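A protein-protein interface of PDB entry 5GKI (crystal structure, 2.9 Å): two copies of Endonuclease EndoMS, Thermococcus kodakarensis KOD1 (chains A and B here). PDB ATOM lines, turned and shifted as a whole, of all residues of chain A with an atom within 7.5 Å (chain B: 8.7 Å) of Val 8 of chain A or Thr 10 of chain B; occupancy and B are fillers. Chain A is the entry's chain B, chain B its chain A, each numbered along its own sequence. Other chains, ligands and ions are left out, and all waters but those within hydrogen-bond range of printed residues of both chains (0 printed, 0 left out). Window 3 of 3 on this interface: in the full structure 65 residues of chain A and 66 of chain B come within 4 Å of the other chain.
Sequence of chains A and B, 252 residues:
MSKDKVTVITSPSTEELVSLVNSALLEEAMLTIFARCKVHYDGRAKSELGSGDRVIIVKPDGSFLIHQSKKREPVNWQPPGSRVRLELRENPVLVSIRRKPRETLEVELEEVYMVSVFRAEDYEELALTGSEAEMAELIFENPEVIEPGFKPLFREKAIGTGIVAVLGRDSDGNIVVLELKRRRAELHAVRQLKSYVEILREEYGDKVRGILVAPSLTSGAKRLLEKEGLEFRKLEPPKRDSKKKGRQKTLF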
ATOM      1  N   VAL A   6      -8.972  -3.909 -28.012  1.00  0.00           N
ATOM      2  CA  VAL A   6      -8.538  -4.010 -26.634  1.00  0.00           C
ATOM      3  C   VAL A   6      -8.858  -5.358 -26.024  1.00  0.00           C
ATOM      4  O   VAL A   6      -9.881  -5.967 -26.325  1.00  0.00           O
ATOM      5  CB  VAL A   6      -9.167  -2.898 -25.783  1.00  0.00           C
ATOM      6  CG1 VAL A   6      -8.599  -2.897 -24.368  1.00  0.00           C
ATOM      7  CG2 VAL A   6      -8.904  -1.567 -26.434  1.00  0.00           C
ATOM      8  N   THR A   7      -7.936  -5.823 -25.190  1.00  0.00           N
ATOM      9  CA  THR A   7      -8.138  -6.998 -24.378  1.00  0.00           C
ATOM     10  C   THR A   7      -7.659  -6.714 -22.939  1.00  0.00           C
ATOM     11  O   THR A   7      -6.484  -6.488 -22.695  1.00  0.00           O
ATOM     12  CB  THR A   7      -7.403  -8.201 -25.000  1.00  0.00           C
ATOM     13  OG1 THR A   7      -7.879  -8.393 -26.339  1.00  0.00           O
ATOM     14  CG2 THR A   7      -7.636  -9.466 -24.189  1.00  0.00           C
ATOM     15  N   VAL A   8      -8.573  -6.724 -21.981  1.00  0.00           N
ATOM     16  CA  VAL A   8      -8.190  -6.408 -20.614  1.00  0.00           C
ATOM     17  C   VAL A   8      -8.415  -7.568 -19.675  1.00  0.00           C
ATOM     18  O   VAL A   8      -9.401  -8.288 -19.800  1.00  0.00           O
ATOM     19  CB  VAL A   8      -8.991  -5.234 -20.049  1.00  0.00           C
ATOM     20  CG1 VAL A   8      -8.166  -4.508 -19.002  1.00  0.00           C
ATOM     21  CG2 VAL A   8      -9.461  -4.305 -21.157  1.00  0.00           C
ATOM     22  N   ILE A   9      -7.509  -7.748 -18.729  1.00  0.00           N
ATOM     23  CA  ILE A   9      -7.773  -8.627 -17.612  1.00  0.00           C
ATOM     24  C   ILE A   9      -7.254  -7.999 -16.338  1.00  0.00           C
ATOM     25  O   ILE A   9      -6.059  -7.745 -16.203  1.00  0.00           O
ATOM     26  CB  ILE A   9      -7.136 -10.010 -17.807  1.00  0.00           C
ATOM     27  CG1 ILE A   9      -7.852 -10.750 -18.941  1.00  0.00           C
ATOM     28  CG2 ILE A   9      -7.220 -10.802 -16.523  1.00  0.00           C
ATOM     29  CD1 ILE A   9      -7.179 -11.990 -19.390  1.00  0.00           C
ATOM     30  N   THR A  10      -8.153  -7.721 -15.408  1.00  0.00           N
ATOM     31  CA  THR A  10      -7.727  -7.288 -14.088  1.00  0.00           C
ATOM     32  C   THR A  10      -7.382  -8.510 -13.235  1.00  0.00           C
ATOM     33  O   THR A  10      -7.820  -9.621 -13.538  1.00  0.00           O
ATOM     34  CB  THR A  10      -8.779  -6.400 -13.428  1.00  0.00           C
ATOM     35  OG1 THR A  10     -10.070  -6.990 -13.567  1.00  0.00           O
ATOM     36  CG2 THR A  10      -8.818  -5.105 -14.153  1.00  0.00           C
ATOM     37  N   PRO A  12      -5.087 -10.762 -13.023  1.00  0.00           N
ATOM     38  CA  PRO A  12      -4.990 -11.953 -13.865  1.00  0.00           C
ATOM     39  C   PRO A  12      -4.200 -13.088 -13.221  1.00  0.00           C
ATOM     40  O   PRO A  12      -3.378 -12.860 -12.326  1.00  0.00           O
ATOM     41  CB  PRO A  12      -4.271 -11.430 -15.100  1.00  0.00           C
ATOM     42  CG  PRO A  12      -3.354 -10.401 -14.549  1.00  0.00           C
ATOM     43  CD  PRO A  12      -4.045  -9.777 -13.363  1.00  0.00           C
ATOM     44  N   GLU A  16      -2.942 -16.225 -17.428  1.00  0.00           N
ATOM     45  CA  GLU A  16      -3.545 -15.151 -18.216  1.00  0.00           C
ATOM     46  C   GLU A  16      -2.502 -14.134 -18.610  1.00  0.00           C
ATOM     47  O   GLU A  16      -2.489 -13.662 -19.752  1.00  0.00           O
ATOM     48  CB  GLU A  16      -4.664 -14.452 -17.450  1.00  0.00           C
ATOM     49  CG  GLU A  16      -5.512 -15.383 -16.653  1.00  0.00           C
ATOM     50  CD  GLU A  16      -6.910 -14.850 -16.428  1.00  0.00           C
ATOM     51  OE1 GLU A  16      -7.158 -14.365 -15.289  1.00  0.00           O
ATOM     52  OE2 GLU A  16      -7.748 -14.928 -17.384  1.00  0.00           O
ATOM     53  N   LEU A  20      -1.589 -13.163 -22.445  1.00  0.00           N
ATOM     54  CA  LEU A  20      -1.734 -11.834 -23.007  1.00  0.00           C
ATOM     55  C   LEU A  20      -0.406 -11.209 -23.408  1.00  0.00           C
ATOM     56  O   LEU A  20      -0.270 -10.690 -24.524  1.00  0.00           O
ATOM     57  CB  LEU A  20      -2.434 -10.928 -22.003  1.00  0.00           C
ATOM     58  CG  LEU A  20      -3.857 -10.553 -22.385  1.00  0.00           C
ATOM     59  CD1 LEU A  20      -4.696 -11.788 -22.425  1.00  0.00           C
ATOM     60  CD2 LEU A  20      -4.411  -9.559 -21.395  1.00  0.00           C
ATOM     61  N   THR A  32      -0.068  -2.714 -22.210  1.00  0.00           N
ATOM     62  CA  THR A  32      -0.098  -1.866 -21.023  1.00  0.00           C
ATOM     63  C   THR A  32      -0.288  -2.725 -19.762  1.00  0.00           C
ATOM     64  O   THR A  32      -1.041  -3.679 -19.786  1.00  0.00           O
ATOM     65  CB  THR A  32      -1.220  -0.834 -21.137  1.00  0.00           C
ATOM     66  OG1 THR A  32      -1.244  -0.321 -22.473  1.00  0.00           O
ATOM     67  CG2 THR A  32      -1.032   0.307 -20.146  1.00  0.00           C
ATOM     68  N   PHE A  34      -0.617  -2.427 -15.207  1.00  0.00           N
ATOM     69  CA  PHE A  34      -0.517  -1.705 -13.935  1.00  0.00           C
ATOM     70  C   PHE A  34      -0.117  -2.708 -12.882  1.00  0.00           C
ATOM     71  O   PHE A  34      -0.806  -3.712 -12.708  1.00  0.00           O
ATOM     72  CB  PHE A  34      -1.825  -1.026 -13.519  1.00  0.00           C
ATOM     73  CG  PHE A  34      -2.498  -0.212 -14.603  1.00  0.00           C
ATOM     74  CD1 PHE A  34      -1.780   0.324 -15.662  1.00  0.00           C
ATOM     75  CD2 PHE A  34      -3.869   0.021 -14.543  1.00  0.00           C
ATOM     76  CE1 PHE A  34      -2.417   1.067 -16.642  1.00  0.00           C
ATOM     77  CE2 PHE A  34      -4.508   0.764 -15.512  1.00  0.00           C
ATOM     78  CZ  PHE A  34      -3.784   1.292 -16.565  1.00  0.00           C
ATOM     79  N   TYR A 113      -2.003  -5.817 -11.283  1.00  0.00           N
ATOM     80  CA  TYR A 113      -3.405  -5.428 -11.136  1.00  0.00           C
ATOM     81  C   TYR A 113      -4.169  -5.490 -12.454  1.00  0.00           C
ATOM     82  O   TYR A 113      -5.375  -5.743 -12.474  1.00  0.00           O
ATOM     83  CB  TYR A 113      -3.525  -4.030 -10.566  1.00  0.00           C
ATOM     84  CG  TYR A 113      -2.715  -3.787  -9.320  1.00  0.00           C
ATOM     85  CD1 TYR A 113      -3.113  -4.311  -8.099  1.00  0.00           C
ATOM     86  CD2 TYR A 113      -1.562  -3.003  -9.357  1.00  0.00           C
ATOM     87  CE1 TYR A 113      -2.375  -4.082  -6.950  1.00  0.00           C
ATOM     88  CE2 TYR A 113      -0.822  -2.759  -8.211  1.00  0.00           C
ATOM     89  CZ  TYR A 113      -1.233  -3.306  -7.008  1.00  0.00           C
ATOM     90  OH  TYR A 113      -0.507  -3.074  -5.860  1.00  0.00           O
ATOM     91  N   MET A 114      -3.475  -5.201 -13.548  1.00  0.00           N
ATOM     92  CA  MET A 114      -4.082  -5.259 -14.866  1.00  0.00           C
ATOM     93  C   MET A 114      -3.067  -5.531 -15.953  1.00  0.00           C
ATOM     94  O   MET A 114      -1.955  -5.015 -15.913  1.00  0.00           O
ATOM     95  CB  MET A 114      -4.804  -3.956 -15.193  1.00  0.00           C
ATOM     96  CG  MET A 114      -5.471  -4.016 -16.534  1.00  0.00           C
ATOM     97  SD  MET A 114      -5.160  -2.600 -17.572  1.00  0.00           S
ATOM     98  CE  MET A 114      -3.386  -2.682 -17.728  1.00  0.00           C
ATOM     99  N   VAL A 115      -3.467  -6.317 -16.942  1.00  0.00           N
ATOM    100  CA  VAL A 115      -2.713  -6.447 -18.179  1.00  0.00           C
ATOM    101  C   VAL A 115      -3.679  -6.152 -19.311  1.00  0.00           C
ATOM    102  O   VAL A 115      -4.879  -6.416 -19.203  1.00  0.00           O
ATOM    103  CB  VAL A 115      -2.085  -7.841 -18.342  1.00  0.00           C
ATOM    104  CG1 VAL A 115      -3.093  -8.920 -17.964  1.00  0.00           C
ATOM    105  CG2 VAL A 115      -1.536  -8.038 -19.766  1.00  0.00           C
ATOM    106  N   SER A 116      -3.170  -5.551 -20.376  1.00  0.00           N
ATOM    107  CA  SER A 116      -4.019  -5.183 -21.484  1.00  0.00           C
ATOM    108  C   SER A 116      -3.235  -5.228 -22.774  1.00  0.00           C
ATOM    109  O   SER A 116      -2.011  -5.061 -22.774  1.00  0.00           O
ATOM    110  CB  SER A 116      -4.616  -3.799 -21.268  1.00  0.00           C
ATOM    111  OG  SER A 116      -3.593  -2.882 -20.937  1.00  0.00           O
ATOM    112  N   VAL A 117      -3.954  -5.493 -23.861  1.00  0.00           N
ATOM    113  CA  VAL A 117      -3.384  -5.459 -25.193  1.00  0.00           C
ATOM    114  C   VAL A 117      -4.205  -4.509 -26.034  1.00  0.00           C
ATOM    115  O   VAL A 117      -5.421  -4.669 -26.192  1.00  0.00           O
ATOM    116  CB  VAL A 117      -3.360  -6.828 -25.871  1.00  0.00           C
ATOM    117  CG1 VAL A 117      -2.704  -6.690 -27.232  1.00  0.00           C
ATOM    118  CG2 VAL A 117      -2.639  -7.860 -25.001  1.00  0.00           C
ATOM    119  N   ARG A 119      -4.607  -3.035 -29.642  1.00  0.00           N
ATOM    120  CA  ARG A 119      -4.152  -3.227 -30.994  1.00  0.00           C
ATOM    121  C   ARG A 119      -4.500  -1.946 -31.720  1.00  0.00           C
ATOM    122  O   ARG A 119      -5.560  -1.801 -32.311  1.00  0.00           O
ATOM    123  CB  ARG A 119      -4.839  -4.449 -31.616  1.00  0.00           C
ATOM    124  CG  ARG A 119      -4.940  -5.643 -30.652  1.00  0.00           C
ATOM    125  CD  ARG A 119      -5.713  -6.851 -31.209  1.00  0.00           C
ATOM    126  NE  ARG A 119      -5.384  -8.071 -30.468  1.00  0.00           N
ATOM    127  CZ  ARG A 119      -5.953  -8.440 -29.320  1.00  0.00           C
ATOM    128  NH1 ARG A 119      -6.902  -7.690 -28.768  1.00  0.00           N
ATOM    129  NH2 ARG A 119      -5.569  -9.564 -28.719  1.00  0.00           N
ATOM    130  N   VAL B   6      -7.799  -0.724  -9.066  1.00  0.00           N
ATOM    131  CA  VAL B   6      -8.045  -0.415 -10.470  1.00  0.00           C
ATOM    132  C   VAL B   6      -9.501  -0.557 -10.894  1.00  0.00           C
ATOM    133  O   VAL B   6     -10.190  -1.505 -10.527  1.00  0.00           O
ATOM    134  CB  VAL B   6      -7.181  -1.309 -11.397  1.00  0.00           C
ATOM    135  CG1 VAL B   6      -7.657  -1.237 -12.854  1.00  0.00           C
ATOM    136  CG2 VAL B   6      -5.720  -0.919 -11.306  1.00  0.00           C
ATOM    137  N   THR B   7      -9.953   0.413 -11.677  1.00  0.00           N
ATOM    138  CA  THR B   7     -11.231   0.367 -12.362  1.00  0.00           C
ATOM    139  C   THR B   7     -11.004   0.431 -13.884  1.00  0.00           C
ATOM    140  O   THR B   7     -10.139   1.153 -14.364  1.00  0.00           O
ATOM    141  CB  THR B   7     -12.124   1.523 -11.914  1.00  0.00           C
ATOM    142  OG1 THR B   7     -11.918   1.773 -10.519  1.00  0.00           O
ATOM    143  CG2 THR B   7     -13.584   1.214 -12.179  1.00  0.00           C
ATOM    144  N   VAL B   8     -11.782  -0.324 -14.637  1.00  0.00           N
ATOM    145  CA  VAL B   8     -11.617  -0.431 -16.078  1.00  0.00           C
ATOM    146  C   VAL B   8     -12.988  -0.474 -16.713  1.00  0.00           C
ATOM    147  O   VAL B   8     -13.842  -1.240 -16.271  1.00  0.00           O
ATOM    148  CB  VAL B   8     -10.862  -1.726 -16.491  1.00  0.00           C
ATOM    149  CG1 VAL B   8     -11.010  -1.991 -17.980  1.00  0.00           C
ATOM    150  CG2 VAL B   8      -9.406  -1.682 -16.081  1.00  0.00           C
ATOM    151  N   ILE B   9     -13.210   0.321 -17.749  1.00  0.00           N
ATOM    152  CA  ILE B   9     -14.414   0.145 -18.546  1.00  0.00           C
ATOM    153  C   ILE B   9     -14.094   0.201 -20.022  1.00  0.00           C
ATOM    154  O   ILE B   9     -13.523   1.169 -20.502  1.00  0.00           O
ATOM    155  CB  ILE B   9     -15.464   1.202 -18.247  1.00  0.00           C
ATOM    156  CG1 ILE B   9     -15.915   1.114 -16.793  1.00  0.00           C
ATOM    157  CG2 ILE B   9     -16.648   1.039 -19.177  1.00  0.00           C
ATOM    158  CD1 ILE B   9     -16.765   2.265 -16.381  1.00  0.00           C
ATOM    159  N   THR B  10     -14.478  -0.841 -20.739  1.00  0.00           N
ATOM    160  CA  THR B  10     -14.290  -0.892 -22.178  1.00  0.00           C
ATOM    161  C   THR B  10     -15.533  -0.397 -22.903  1.00  0.00           C
ATOM    162  O   THR B  10     -16.655  -0.657 -22.466  1.00  0.00           O
ATOM    163  CB  THR B  10     -13.967  -2.307 -22.619  1.00  0.00           C
ATOM    164  OG1 THR B  10     -15.022  -3.179 -22.186  1.00  0.00           O
ATOM    165  CG2 THR B  10     -12.669  -2.747 -21.975  1.00  0.00           C
ATOM    166  N   SER B  11     -15.316   0.288 -24.023  1.00  0.00           N
ATOM    167  CA  SER B  11     -16.369   0.980 -24.771  1.00  0.00           C
ATOM    168  C   SER B  11     -17.304   1.704 -23.821  1.00  0.00           C
ATOM    169  O   SER B  11     -18.474   1.342 -23.708  1.00  0.00           O
ATOM    170  CB  SER B  11     -17.159   0.002 -25.634  1.00  0.00           C
ATOM    171  OG  SER B  11     -16.306  -0.919 -26.290  1.00  0.00           O
ATOM    172  N   PRO B  12     -16.786   2.709 -23.102  1.00  0.00           N
ATOM    173  CA  PRO B  12     -17.636   3.366 -22.113  1.00  0.00           C
ATOM    174  C   PRO B  12     -18.636   4.304 -22.748  1.00  0.00           C
ATOM    175  O   PRO B  12     -18.402   4.826 -23.838  1.00  0.00           O
ATOM    176  CB  PRO B  12     -16.641   4.148 -21.261  1.00  0.00           C
ATOM    177  CG  PRO B  12     -15.545   4.443 -22.174  1.00  0.00           C
ATOM    178  CD  PRO B  12     -15.433   3.286 -23.118  1.00  0.00           C
ATOM    179  N   SER B  13     -19.755   4.480 -22.061  1.00  0.00           N
ATOM    180  CA  SER B  13     -20.691   5.547 -22.346  1.00  0.00           C
ATOM    181  C   SER B  13     -20.100   6.863 -21.862  1.00  0.00           C
ATOM    182  O   SER B  13     -19.204   6.871 -21.012  1.00  0.00           O
ATOM    183  CB  SER B  13     -22.009   5.295 -21.640  1.00  0.00           C
ATOM    184  OG  SER B  13     -21.795   5.346 -20.235  1.00  0.00           O
ATOM    185  N   GLU B  16     -20.182   7.061 -18.218  1.00  0.00           N
ATOM    186  CA  GLU B  16     -19.108   6.236 -17.643  1.00  0.00           C
ATOM    187  C   GLU B  16     -17.751   6.932 -17.796  1.00  0.00           C
ATOM    188  O   GLU B  16     -17.008   7.069 -16.814  1.00  0.00           O
ATOM    189  CB  GLU B  16     -19.054   4.842 -18.282  1.00  0.00           C
ATOM    190  CG  GLU B  16     -20.244   3.951 -17.954  1.00  0.00           C
ATOM    191  CD  GLU B  16     -20.292   2.647 -18.764  1.00  0.00           C
ATOM    192  OE1 GLU B  16     -20.099   2.692 -20.005  1.00  0.00           O
ATOM    193  OE2 GLU B  16     -20.539   1.574 -18.154  1.00  0.00           O
ATOM    194  N   LEU B  20     -15.441   8.183 -14.608  1.00  0.00           N
ATOM    195  CA  LEU B  20     -14.098   7.707 -14.328  1.00  0.00           C
ATOM    196  C   LEU B  20     -13.070   8.816 -14.310  1.00  0.00           C
ATOM    197  O   LEU B  20     -12.350   8.972 -13.319  1.00  0.00           O
ATOM    198  CB  LEU B  20     -13.690   6.657 -15.343  1.00  0.00           C
ATOM    199  CG  LEU B  20     -13.603   5.277 -14.692  1.00  0.00           C
ATOM    200  CD1 LEU B  20     -14.969   4.835 -14.204  1.00  0.00           C
ATOM    201  CD2 LEU B  20     -13.016   4.268 -15.652  1.00  0.00           C
ATOM    202  N   PHE B  34      -7.360   4.360 -23.745  1.00  0.00           N
ATOM    203  CA  PHE B  34      -7.072   3.912 -25.101  1.00  0.00           C
ATOM    204  C   PHE B  34      -8.136   4.490 -26.008  1.00  0.00           C
ATOM    205  O   PHE B  34      -9.311   4.187 -25.845  1.00  0.00           O
ATOM    206  CB  PHE B  34      -7.077   2.382 -25.219  1.00  0.00           C
ATOM    207  CG  PHE B  34      -6.119   1.685 -24.297  1.00  0.00           C
ATOM    208  CD1 PHE B  34      -5.093   2.376 -23.676  1.00  0.00           C
ATOM    209  CD2 PHE B  34      -6.240   0.329 -24.070  1.00  0.00           C
ATOM    210  CE1 PHE B  34      -4.217   1.730 -22.825  1.00  0.00           C
ATOM    211  CE2 PHE B  34      -5.381  -0.325 -23.221  1.00  0.00           C
ATOM    212  CZ  PHE B  34      -4.363   0.376 -22.594  1.00  0.00           C
ATOM    213  N   GLU B 111     -13.478   7.924 -30.475  1.00  0.00           N
ATOM    214  CA  GLU B 111     -13.924   6.627 -29.974  1.00  0.00           C
ATOM    215  C   GLU B 111     -13.078   6.191 -28.775  1.00  0.00           C
ATOM    216  O   GLU B 111     -11.886   5.959 -28.921  1.00  0.00           O
ATOM    217  CB  GLU B 111     -13.840   5.582 -31.091  1.00  0.00           C
ATOM    218  CG  GLU B 111     -15.179   5.208 -31.701  1.00  0.00           C
ATOM    219  CD  GLU B 111     -15.935   4.236 -30.828  1.00  0.00           C
ATOM    220  OE1 GLU B 111     -15.314   3.220 -30.441  1.00  0.00           O
ATOM    221  OE2 GLU B 111     -17.124   4.496 -30.515  1.00  0.00           O
ATOM    222  N   VAL B 112     -13.670   6.060 -27.598  1.00  0.00           N
ATOM    223  CA  VAL B 112     -12.891   5.560 -26.466  1.00  0.00           C
ATOM    224  C   VAL B 112     -12.999   4.028 -26.321  1.00  0.00           C
ATOM    225  O   VAL B 112     -14.047   3.494 -25.980  1.00  0.00           O
ATOM    226  CB  VAL B 112     -13.333   6.208 -25.142  1.00  0.00           C
ATOM    227  CG1 VAL B 112     -12.600   5.568 -23.970  1.00  0.00           C
ATOM    228  CG2 VAL B 112     -13.107   7.712 -25.171  1.00  0.00           C
ATOM    229  N   TYR B 113     -11.913   3.313 -26.569  1.00  0.00           N
ATOM    230  CA  TYR B 113     -11.956   1.859 -26.472  1.00  0.00           C
ATOM    231  C   TYR B 113     -11.848   1.390 -25.025  1.00  0.00           C
ATOM    232  O   TYR B 113     -12.451   0.396 -24.647  1.00  0.00           O
ATOM    233  CB  TYR B 113     -10.837   1.215 -27.301  1.00  0.00           C
ATOM    234  CG  TYR B 113     -10.677   1.775 -28.694  1.00  0.00           C
ATOM    235  CD1 TYR B 113     -11.642   1.552 -29.667  1.00  0.00           C
ATOM    236  CD2 TYR B 113      -9.558   2.530 -29.037  1.00  0.00           C
ATOM    237  CE1 TYR B 113     -11.504   2.055 -30.942  1.00  0.00           C
ATOM    238  CE2 TYR B 113      -9.413   3.037 -30.312  1.00  0.00           C
ATOM    239  CZ  TYR B 113     -10.393   2.794 -31.257  1.00  0.00           C
ATOM    240  OH  TYR B 113     -10.271   3.290 -32.528  1.00  0.00           O
ATOM    241  N   MET B 114     -11.061   2.084 -24.218  1.00  0.00           N
ATOM    242  CA  MET B 114     -10.964   1.753 -22.800  1.00  0.00           C
ATOM    243  C   MET B 114     -10.624   2.992 -21.978  1.00  0.00           C
ATOM    244  O   MET B 114      -9.911   3.889 -22.436  1.00  0.00           O
ATOM    245  CB  MET B 114      -9.919   0.658 -22.561  1.00  0.00           C
ATOM    246  CG  MET B 114      -9.910   0.103 -21.136  1.00  0.00           C
ATOM    247  SD  MET B 114      -8.288  -0.467 -20.552  1.00  0.00           S
ATOM    248  CE  MET B 114      -7.404   1.101 -20.572  1.00  0.00           C
ATOM    249  N   VAL B 115     -11.153   3.039 -20.764  1.00  0.00           N
ATOM    250  CA  VAL B 115     -10.803   4.075 -19.812  1.00  0.00           C
ATOM    251  C   VAL B 115     -10.492   3.337 -18.541  1.00  0.00           C
ATOM    252  O   VAL B 115     -11.068   2.281 -18.281  1.00  0.00           O
ATOM    253  CB  VAL B 115     -11.936   5.122 -19.603  1.00  0.00           C
ATOM    254  CG1 VAL B 115     -13.233   4.455 -19.167  1.00  0.00           C
ATOM    255  CG2 VAL B 115     -11.520   6.152 -18.588  1.00  0.00           C
ATOM    256  N   SER B 116      -9.542   3.842 -17.771  1.00  0.00           N
ATOM    257  CA  SER B 116      -9.179   3.163 -16.542  1.00  0.00           C
ATOM    258  C   SER B 116      -8.638   4.106 -15.495  1.00  0.00           C
ATOM    259  O   SER B 116      -7.899   5.049 -15.796  1.00  0.00           O
ATOM    260  CB  SER B 116      -8.154   2.069 -16.822  1.00  0.00           C
ATOM    261  OG  SER B 116      -6.961   2.631 -17.328  1.00  0.00           O
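SD of Met 114 of chain A sits close to OG of Ser 116 of chain A (3.7 Å).
The backbone NH of Tyr 113 of chain A lies within hydrogen-bond range of the backbone carbonyl oxygen of Phe 34 of chain A (2.8 Å).
N of Phe 34 of chain B sits at hydrogen-bond distance from O of Met 114 of chain B (2.9 Å).
The backbone carbonyl oxygen of Met 114 of chain A is in hydrogen-bond range of the backbone NH of Phe 34 of chain A.
O of Thr 32 of chain A is in hydrogen-bond range of N of Ser 116 of chain A, at 2.9 Å.
O of Phe 34 of chain B lies within hydrogen-bond range of N of Tyr 113 of chain B (2.8 Å).
Val 6 of chain A touches Tyr 113 of chain B (CG2 to CB, 3.5 Å).
Val 8 of chain A touches Val 8 of chain B (CG1 to CG1, 3.9 Å).
Val 8 of chain A touches Thr 10 of chain B (CG2 to CG2, 3.7 Å).
Thr 10 of chain A touches Val 8 of chain B.
Thr 32 of chain A touches Phe 34 of chain B.
Phe 34 of chain A touches Val 6 of chain B.
Phe 34 of chain A touches Ser 116 of chain B.
Tyr 113 of chain A touches Val 6 of chain B (CB to CG2, 3.9 Å).
Ser 116 of chain A touches Phe 34 of chain B.
Printed residues of chain B within 4 Å of Val 6 of chain A: Tyr 113.
Printed residues of chain B within 4 Å of Val 8 of chain A: Val 8 and Thr 10.
Of the printed residues of chain B, Ser 116 of chain A touches Phe 34.
Printed residues of chain A within 4 Å of Val 6 of chain B: Phe 34 (3.8 Å) and Tyr 113 (3.9 Å).
Ile 9 of chain B touches none of the printed residues of chain A.
Of chain A, only Val 8 comes within 4 Å of Thr 10 of chain B.
Printed residues of chain A within 4 Å of Phe 34 of chain B: Thr 32 and Ser 116.
The nearest residue of chain B that does not touch Val 8 of chain A is Met 114 of chain B (4.1 Å).
The nearest residue of chain A that does not touch Thr 10 of chain B is Val 6 of chain A (4.7 Å).
Along chain B the printed residues that touch a printed residue of chain A span positions 6 to 116.
Among the printed residues, 9 pairs touch across the chains.
Among the printed residues, no Asp or Glu carboxylate lies within 4 Å of a Lys or Arg side-chain nitrogen of the other chain.
Val 6 of chain A touches Tyr 113 of chain B, and with the chains exchanged Tyr 113 of chain A touches Val 6 of chain B.
Val 8 of chain A touches its own counterpart, Val 8 of chain B.
Val 8 of chain A touches Thr 10 of chain B, and with the chains exchanged Thr 10 of chain A touches Val 8 of chain B.
Phe 34 of chain A touches Val 6 of chain B, but with the chains exchanged Val 6 of chain A does not touch Phe 34 of chain B (4.01 Å).
13 positions are printed for both chains.
Of the 9 pairs that touch across the chains among the printed residues, 7 have their exchanged pair printed and touching as well.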
